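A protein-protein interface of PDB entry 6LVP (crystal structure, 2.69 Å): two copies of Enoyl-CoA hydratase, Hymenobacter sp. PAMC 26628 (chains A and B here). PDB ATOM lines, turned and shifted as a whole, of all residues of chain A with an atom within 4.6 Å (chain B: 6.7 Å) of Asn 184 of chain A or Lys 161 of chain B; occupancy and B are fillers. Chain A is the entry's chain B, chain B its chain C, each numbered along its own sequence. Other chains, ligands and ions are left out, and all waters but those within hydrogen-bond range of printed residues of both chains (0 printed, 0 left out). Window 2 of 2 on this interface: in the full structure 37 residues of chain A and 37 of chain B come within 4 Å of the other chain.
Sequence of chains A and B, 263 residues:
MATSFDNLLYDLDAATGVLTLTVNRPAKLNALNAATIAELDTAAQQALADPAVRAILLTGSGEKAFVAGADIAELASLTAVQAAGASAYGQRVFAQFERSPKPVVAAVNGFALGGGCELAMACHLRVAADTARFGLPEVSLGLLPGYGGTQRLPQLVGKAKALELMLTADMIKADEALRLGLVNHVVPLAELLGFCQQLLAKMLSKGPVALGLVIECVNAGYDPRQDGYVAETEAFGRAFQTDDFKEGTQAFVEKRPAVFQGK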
ATOM      1  N   LEU A 125       1.179 -20.795  -5.147  1.00  0.00           N
ATOM      2  CA  LEU A 125       0.900 -21.153  -6.531  1.00  0.00           C
ATOM      3  C   LEU A 125      -0.604 -21.347  -6.696  1.00  0.00           C
ATOM      4  O   LEU A 125      -1.295 -21.770  -5.766  1.00  0.00           O
ATOM      5  CB  LEU A 125       1.668 -22.428  -6.935  1.00  0.00           C
ATOM      6  CG  LEU A 125       3.131 -22.457  -7.429  1.00  0.00           C
ATOM      7  CD1 LEU A 125       4.030 -21.381  -6.851  1.00  0.00           C
ATOM      8  CD2 LEU A 125       3.760 -23.828  -7.178  1.00  0.00           C
ATOM      9  N   ARG A 126      -1.115 -21.002  -7.877  1.00  0.00           N
ATOM     10  CA  ARG A 126      -2.509 -21.244  -8.231  1.00  0.00           C
ATOM     11  C   ARG A 126      -2.552 -22.015  -9.542  1.00  0.00           C
ATOM     12  O   ARG A 126      -1.940 -21.591 -10.527  1.00  0.00           O
ATOM     13  CB  ARG A 126      -3.291 -19.930  -8.357  1.00  0.00           C
ATOM     14  CG  ARG A 126      -3.735 -19.327  -7.032  1.00  0.00           C
ATOM     15  CD  ARG A 126      -3.650 -17.786  -7.009  1.00  0.00           C
ATOM     16  NE  ARG A 126      -2.333 -17.307  -7.424  1.00  0.00           N
ATOM     17  CZ  ARG A 126      -1.252 -17.267  -6.648  1.00  0.00           C
ATOM     18  NH1 ARG A 126      -1.305 -17.667  -5.383  1.00  0.00           N
ATOM     19  NH2 ARG A 126      -0.104 -16.829  -7.145  1.00  0.00           N
ATOM     20  N   LEU A 178      -4.763 -16.440 -16.338  1.00  0.00           N
ATOM     21  CA  LEU A 178      -3.466 -16.973 -16.775  1.00  0.00           C
ATOM     22  C   LEU A 178      -3.059 -16.219 -18.028  1.00  0.00           C
ATOM     23  O   LEU A 178      -3.264 -16.670 -19.153  1.00  0.00           O
ATOM     24  CB  LEU A 178      -3.556 -18.471 -17.038  1.00  0.00           C
ATOM     25  CG  LEU A 178      -2.368 -19.348 -17.459  1.00  0.00           C
ATOM     26  CD1 LEU A 178      -2.273 -19.497 -18.963  1.00  0.00           C
ATOM     27  CD2 LEU A 178      -1.072 -18.834 -16.878  1.00  0.00           C
ATOM     28  N   LEU A 182      -2.461 -14.176 -12.567  1.00  0.00           N
ATOM     29  CA  LEU A 182      -3.243 -14.527 -11.391  1.00  0.00           C
ATOM     30  C   LEU A 182      -3.316 -16.029 -11.163  1.00  0.00           C
ATOM     31  O   LEU A 182      -3.573 -16.462 -10.039  1.00  0.00           O
ATOM     32  CB  LEU A 182      -4.646 -13.930 -11.513  1.00  0.00           C
ATOM     33  CG  LEU A 182      -5.628 -14.127 -10.356  1.00  0.00           C
ATOM     34  CD1 LEU A 182      -5.034 -13.640  -9.041  1.00  0.00           C
ATOM     35  CD2 LEU A 182      -6.924 -13.417 -10.661  1.00  0.00           C
ATOM     36  N   VAL A 183      -3.107 -16.846 -12.183  1.00  0.00           N
ATOM     37  CA  VAL A 183      -2.855 -18.259 -11.945  1.00  0.00           C
ATOM     38  C   VAL A 183      -1.644 -18.634 -12.768  1.00  0.00           C
ATOM     39  O   VAL A 183      -1.277 -17.938 -13.719  1.00  0.00           O
ATOM     40  CB  VAL A 183      -4.046 -19.198 -12.281  1.00  0.00           C
ATOM     41  CG1 VAL A 183      -5.366 -18.594 -11.813  1.00  0.00           C
ATOM     42  CG2 VAL A 183      -4.078 -19.550 -13.755  1.00  0.00           C
ATOM     43  N   ASN A 184      -1.014 -19.744 -12.368  1.00  0.00           N
ATOM     44  CA  ASN A 184       0.191 -20.252 -13.010  1.00  0.00           C
ATOM     45  C   ASN A 184      -0.109 -21.176 -14.177  1.00  0.00           C
ATOM     46  O   ASN A 184       0.695 -21.260 -15.116  1.00  0.00           O
ATOM     47  CB  ASN A 184       1.044 -20.999 -11.986  1.00  0.00           C
ATOM     48  CG  ASN A 184       1.557 -20.083 -10.872  1.00  0.00           C
ATOM     49  OD1 ASN A 184       0.782 -19.579 -10.043  1.00  0.00           O
ATOM     50  ND2 ASN A 184       2.872 -19.866 -10.850  1.00  0.00           N
ATOM     51  N   HIS A 185      -1.247 -21.867 -14.132  1.00  0.00           N
ATOM     52  CA  HIS A 185      -1.578 -22.922 -15.077  1.00  0.00           C
ATOM     53  C   HIS A 185      -3.088 -23.099 -15.112  1.00  0.00           C
ATOM     54  O   HIS A 185      -3.759 -22.961 -14.089  1.00  0.00           O
ATOM     55  CB  HIS A 185      -0.910 -24.241 -14.680  1.00  0.00           C
ATOM     56  CG  HIS A 185       0.578 -24.243 -14.841  1.00  0.00           C
ATOM     57  ND1 HIS A 185       1.194 -24.131 -16.068  1.00  0.00           N
ATOM     58  CD2 HIS A 185       1.574 -24.363 -13.931  1.00  0.00           C
ATOM     59  CE1 HIS A 185       2.502 -24.194 -15.909  1.00  0.00           C
ATOM     60  NE2 HIS A 185       2.760 -24.336 -14.621  1.00  0.00           N
ATOM     61  N   LEU B 153      14.362 -12.071  -9.435  1.00  0.00           N
ATOM     62  CA  LEU B 153      13.405 -12.845 -10.227  1.00  0.00           C
ATOM     63  C   LEU B 153      11.969 -12.361 -10.031  1.00  0.00           C
ATOM     64  O   LEU B 153      11.272 -12.145 -11.038  1.00  0.00           O
ATOM     65  CB  LEU B 153      13.554 -14.339  -9.927  1.00  0.00           C
ATOM     66  CG  LEU B 153      12.766 -15.269 -10.850  1.00  0.00           C
ATOM     67  CD1 LEU B 153      13.046 -14.954 -12.306  1.00  0.00           C
ATOM     68  CD2 LEU B 153      13.088 -16.727 -10.542  1.00  0.00           C
ATOM     69  N   VAL B 157       9.489 -11.252 -13.304  1.00  0.00           N
ATOM     70  CA  VAL B 157       8.446 -12.143 -13.808  1.00  0.00           C
ATOM     71  C   VAL B 157       7.292 -12.272 -12.822  1.00  0.00           C
ATOM     72  O   VAL B 157       6.358 -13.051 -13.052  1.00  0.00           O
ATOM     73  CB  VAL B 157       9.001 -13.542 -14.162  1.00  0.00           C
ATOM     74  CG1 VAL B 157      10.187 -13.442 -15.125  1.00  0.00           C
ATOM     75  CG2 VAL B 157       9.350 -14.340 -12.901  1.00  0.00           C
ATOM     76  N   GLY B 158       7.340 -11.523 -11.726  1.00  0.00           N
ATOM     77  CA  GLY B 158       6.277 -11.542 -10.746  1.00  0.00           C
ATOM     78  C   GLY B 158       6.479 -12.582  -9.647  1.00  0.00           C
ATOM     79  O   GLY B 158       7.310 -13.497  -9.728  1.00  0.00           O
ATOM     80  N   LYS B 159       5.665 -12.437  -8.603  1.00  0.00           N
ATOM     81  CA  LYS B 159       5.757 -13.302  -7.437  1.00  0.00           C
ATOM     82  C   LYS B 159       5.507 -14.763  -7.802  1.00  0.00           C
ATOM     83  O   LYS B 159       6.319 -15.644  -7.489  1.00  0.00           O
ATOM     84  CB  LYS B 159       4.747 -12.821  -6.389  1.00  0.00           C
ATOM     85  CG  LYS B 159       5.148 -12.958  -4.925  1.00  0.00           C
ATOM     86  CD  LYS B 159       3.897 -13.198  -4.108  1.00  0.00           C
ATOM     87  CE  LYS B 159       4.002 -12.712  -2.677  1.00  0.00           C
ATOM     88  NZ  LYS B 159       2.631 -12.631  -2.049  1.00  0.00           N
ATOM     89  N   ALA B 160       4.380 -15.039  -8.461  1.00  0.00           N
ATOM     90  CA  ALA B 160       3.932 -16.416  -8.656  1.00  0.00           C
ATOM     91  C   ALA B 160       4.930 -17.227  -9.480  1.00  0.00           C
ATOM     92  O   ALA B 160       5.294 -18.356  -9.118  1.00  0.00           O
ATOM     93  CB  ALA B 160       2.559 -16.410  -9.316  1.00  0.00           C
ATOM     94  N   LYS B 161       5.391 -16.669 -10.591  1.00  0.00           N
ATOM     95  CA  LYS B 161       6.287 -17.439 -11.429  1.00  0.00           C
ATOM     96  C   LYS B 161       7.705 -17.463 -10.871  1.00  0.00           C
ATOM     97  O   LYS B 161       8.455 -18.406 -11.149  1.00  0.00           O
ATOM     98  CB  LYS B 161       6.263 -16.891 -12.850  1.00  0.00           C
ATOM     99  CG  LYS B 161       5.770 -17.893 -13.874  1.00  0.00           C
ATOM    100  CD  LYS B 161       4.283 -18.070 -13.827  1.00  0.00           C
ATOM    101  CE  LYS B 161       3.806 -19.076 -14.883  1.00  0.00           C
ATOM    102  NZ  LYS B 161       4.214 -20.474 -14.577  1.00  0.00           N
ATOM    103  N   ALA B 162       8.097 -16.460 -10.080  1.00  0.00           N
ATOM    104  CA  ALA B 162       9.378 -16.551  -9.384  1.00  0.00           C
ATOM    105  C   ALA B 162       9.358 -17.695  -8.382  1.00  0.00           C
ATOM    106  O   ALA B 162      10.297 -18.499  -8.319  1.00  0.00           O
ATOM    107  CB  ALA B 162       9.712 -15.233  -8.691  1.00  0.00           C
ATOM    108  N   LEU B 163       8.282 -17.795  -7.595  1.00  0.00           N
ATOM    109  CA  LEU B 163       8.143 -18.933  -6.694  1.00  0.00           C
ATOM    110  C   LEU B 163       8.168 -20.253  -7.462  1.00  0.00           C
ATOM    111  O   LEU B 163       8.939 -21.161  -7.125  1.00  0.00           O
ATOM    112  CB  LEU B 163       6.866 -18.798  -5.859  1.00  0.00           C
ATOM    113  CG  LEU B 163       6.966 -17.792  -4.696  1.00  0.00           C
ATOM    114  CD1 LEU B 163       5.655 -17.580  -3.997  1.00  0.00           C
ATOM    115  CD2 LEU B 163       8.015 -18.227  -3.700  1.00  0.00           C
ATOM    116  N   GLU B 164       7.353 -20.379  -8.514  1.00  0.00           N
ATOM    117  CA  GLU B 164       7.324 -21.652  -9.225  1.00  0.00           C
ATOM    118  C   GLU B 164       8.716 -22.040  -9.703  1.00  0.00           C
ATOM    119  O   GLU B 164       9.188 -23.152  -9.433  1.00  0.00           O
ATOM    120  CB  GLU B 164       6.347 -21.617 -10.402  1.00  0.00           C
ATOM    121  CG  GLU B 164       6.304 -22.964 -11.122  1.00  0.00           C
ATOM    122  CD  GLU B 164       5.306 -23.053 -12.262  1.00  0.00           C
ATOM    123  OE1 GLU B 164       4.631 -22.040 -12.560  1.00  0.00           O
ATOM    124  OE2 GLU B 164       5.214 -24.159 -12.860  1.00  0.00           O
ATOM    125  N   LEU B 165       9.412 -21.124 -10.377  1.00  0.00           N
ATOM    126  CA  LEU B 165      10.725 -21.466 -10.908  1.00  0.00           C
ATOM    127  C   LEU B 165      11.711 -21.823  -9.792  1.00  0.00           C
ATOM    128  O   LEU B 165      12.528 -22.744  -9.944  1.00  0.00           O
ATOM    129  CB  LEU B 165      11.256 -20.315 -11.758  1.00  0.00           C
ATOM    130  CG  LEU B 165      10.725 -20.198 -13.186  1.00  0.00           C
ATOM    131  CD1 LEU B 165      10.901 -18.789 -13.716  1.00  0.00           C
ATOM    132  CD2 LEU B 165      11.424 -21.186 -14.114  1.00  0.00           C
ATOM    133  N   MET B 166      11.668 -21.104  -8.666  1.00  0.00           N
ATOM    134  CA  MET B 166      12.623 -21.376  -7.601  1.00  0.00           C
ATOM    135  C   MET B 166      12.207 -22.548  -6.717  1.00  0.00           C
ATOM    136  O   MET B 166      13.071 -23.157  -6.079  1.00  0.00           O
ATOM    137  CB  MET B 166      12.836 -20.120  -6.755  1.00  0.00           C
ATOM    138  CG  MET B 166      13.794 -19.107  -7.382  1.00  0.00           C
ATOM    139  SD  MET B 166      13.985 -17.572  -6.419  1.00  0.00           S
ATOM    140  CE  MET B 166      12.312 -16.931  -6.396  1.00  0.00           C
ATOM    141  N   GLU B 176       9.631 -18.901 -23.408  1.00  0.00           N
ATOM    142  CA  GLU B 176       8.940 -18.761 -22.123  1.00  0.00           C
ATOM    143  C   GLU B 176       9.483 -17.576 -21.332  1.00  0.00           C
ATOM    144  O   GLU B 176       8.716 -16.776 -20.778  1.00  0.00           O
ATOM    145  CB  GLU B 176       9.084 -20.040 -21.297  1.00  0.00           C
ATOM    146  CG  GLU B 176       7.827 -20.870 -21.165  1.00  0.00           C
ATOM    147  CD  GLU B 176       6.639 -20.081 -20.641  1.00  0.00           C
ATOM    148  OE1 GLU B 176       5.855 -19.560 -21.469  1.00  0.00           O
ATOM    149  OE2 GLU B 176       6.486 -19.989 -19.403  1.00  0.00           O
ATOM    150  N   ARG B 179       8.031 -14.469 -22.706  1.00  0.00           N
ATOM    151  CA  ARG B 179       6.639 -14.334 -22.277  1.00  0.00           C
ATOM    152  C   ARG B 179       6.529 -13.940 -20.799  1.00  0.00           C
ATOM    153  O   ARG B 179       5.647 -13.158 -20.425  1.00  0.00           O
ATOM    154  CB  ARG B 179       5.902 -15.649 -22.559  1.00  0.00           C
ATOM    155  CG  ARG B 179       4.395 -15.559 -22.763  1.00  0.00           C
ATOM    156  CD  ARG B 179       3.695 -16.898 -22.457  1.00  0.00           C
ATOM    157  NE  ARG B 179       3.313 -17.025 -21.043  1.00  0.00           N
ATOM    158  CZ  ARG B 179       3.242 -18.180 -20.381  1.00  0.00           C
ATOM    159  NH1 ARG B 179       3.534 -19.316 -21.000  1.00  0.00           N
ATOM    160  NH2 ARG B 179       2.891 -18.202 -19.096  1.00  0.00           N
ATOM    161  N   LEU B 180       7.414 -14.468 -19.940  1.00  0.00           N
ATOM    162  CA  LEU B 180       7.384 -14.101 -18.524  1.00  0.00           C
ATOM    163  C   LEU B 180       8.015 -12.736 -18.241  1.00  0.00           C
ATOM    164  O   LEU B 180       7.717 -12.140 -17.204  1.00  0.00           O
ATOM    165  CB  LEU B 180       8.080 -15.170 -17.654  1.00  0.00           C
ATOM    166  CG  LEU B 180       7.527 -16.621 -17.574  1.00  0.00           C
ATOM    167  CD1 LEU B 180       8.408 -17.550 -16.703  1.00  0.00           C
ATOM    168  CD2 LEU B 180       6.030 -16.735 -17.123  1.00  0.00           C
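The guanidinium group of Arg 126 of chain A lies within hydrogen-bond range of the backbone carbonyl oxygen of Leu 182 of chain A (3.0 Å). The backbone carbonyl oxygen (O) of Arg 126 of chain A sits at hydrogen-bond distance from the backbone NH (N) of Asn 184 of chain A, 2.8 Å away. The side-chain carboxylate (OE1) of Glu 164 of chain B lies within salt-bridge range of the side-chain amino group (NZ) of Lys 161 of chain B.
No position is printed for both chains. Of the 8 pairs that touch across the chains among the printed residues, none has its exchanged pair printed and touching as well.
The backbone carbonyl oxygen of Ala 160 of chain B lies within hydrogen-bond range of the side-chain amide nitrogen of Asn 184 of chain A (3.3 Å). The side-chain carboxylate (OE1) of Glu 164 of chain B is in hydrogen-bond range of the side-chain amide nitrogen (ND2) of Asn 184 of chain A, at 3.3 Å. A ring nitrogen (NE2) of His 185 of chain A lies within hydrogen-bond range of the side-chain carboxylate (OE2) of Glu 164 of chain B (3.0 Å).
Among the printed residues, merely in contact across the chains: Arg 126 of chain A with Ala 160 of chain B (3.5 Å), Asn 184 of chain A with Lys 161 of chain B (3.6 Å), Leu 125 of chain A with Glu 164 of chain B (3.8 Å), Leu 125 of chain A with Leu 163 of chain B (3.96 Å) and Leu 125 of chain A with Ala 160 of chain B (3.99 Å).
Of the 7 printed residues of chain A, 4 touch a printed residue of chain B. Hydrophobic or aromatic side chains of chain A within 4 Å of the printed part of chain B: Leu 125 and His 185. Hydrophobic or aromatic side chains of chain B that line the printed part of chain A: Ala 160 and Leu 163. Among the printed residues, no Asp or Glu carboxylate lies within 4 Å of a Lys or Arg side-chain nitrogen of the other chain.
Of the printed residues of chain B, Leu 125 of chain A touches Ala 160 (3.99 Å), Leu 163 (3.96 Å) and Glu 164 (3.8 Å). Printed residues of chain B within 4 Å of Arg 126 of chain A: Ala 160. Val 183 of chain A touches none of the printed residues of chain B. Asn 184 of chain A touches just these residues of chain B: Ala 160 (3.3 Å), Lys 161 (3.6 Å) and Glu 164 (3.3 Å). Of the printed residues of chain B, His 185 of chain A touches Glu 164. Printed residues of chain A within 4 Å of Ala 160 of chain B: Leu 125 (3.99 Å), Arg 126 (3.5 Å) and Asn 184 (3.3 Å). Of chain A, only Asn 184 (3.6 Å) comes within 4 Å of Lys 161 of chain B. Of the printed residues of chain A, Leu 163 of chain B touches Leu 125 (3.96 Å). Glu 176 of chain B touches none of the printed residues of chain A. The nearest printed residue of chain B that does not touch His 185 of chain A is Lys 161 of chain B (4.1 Å).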
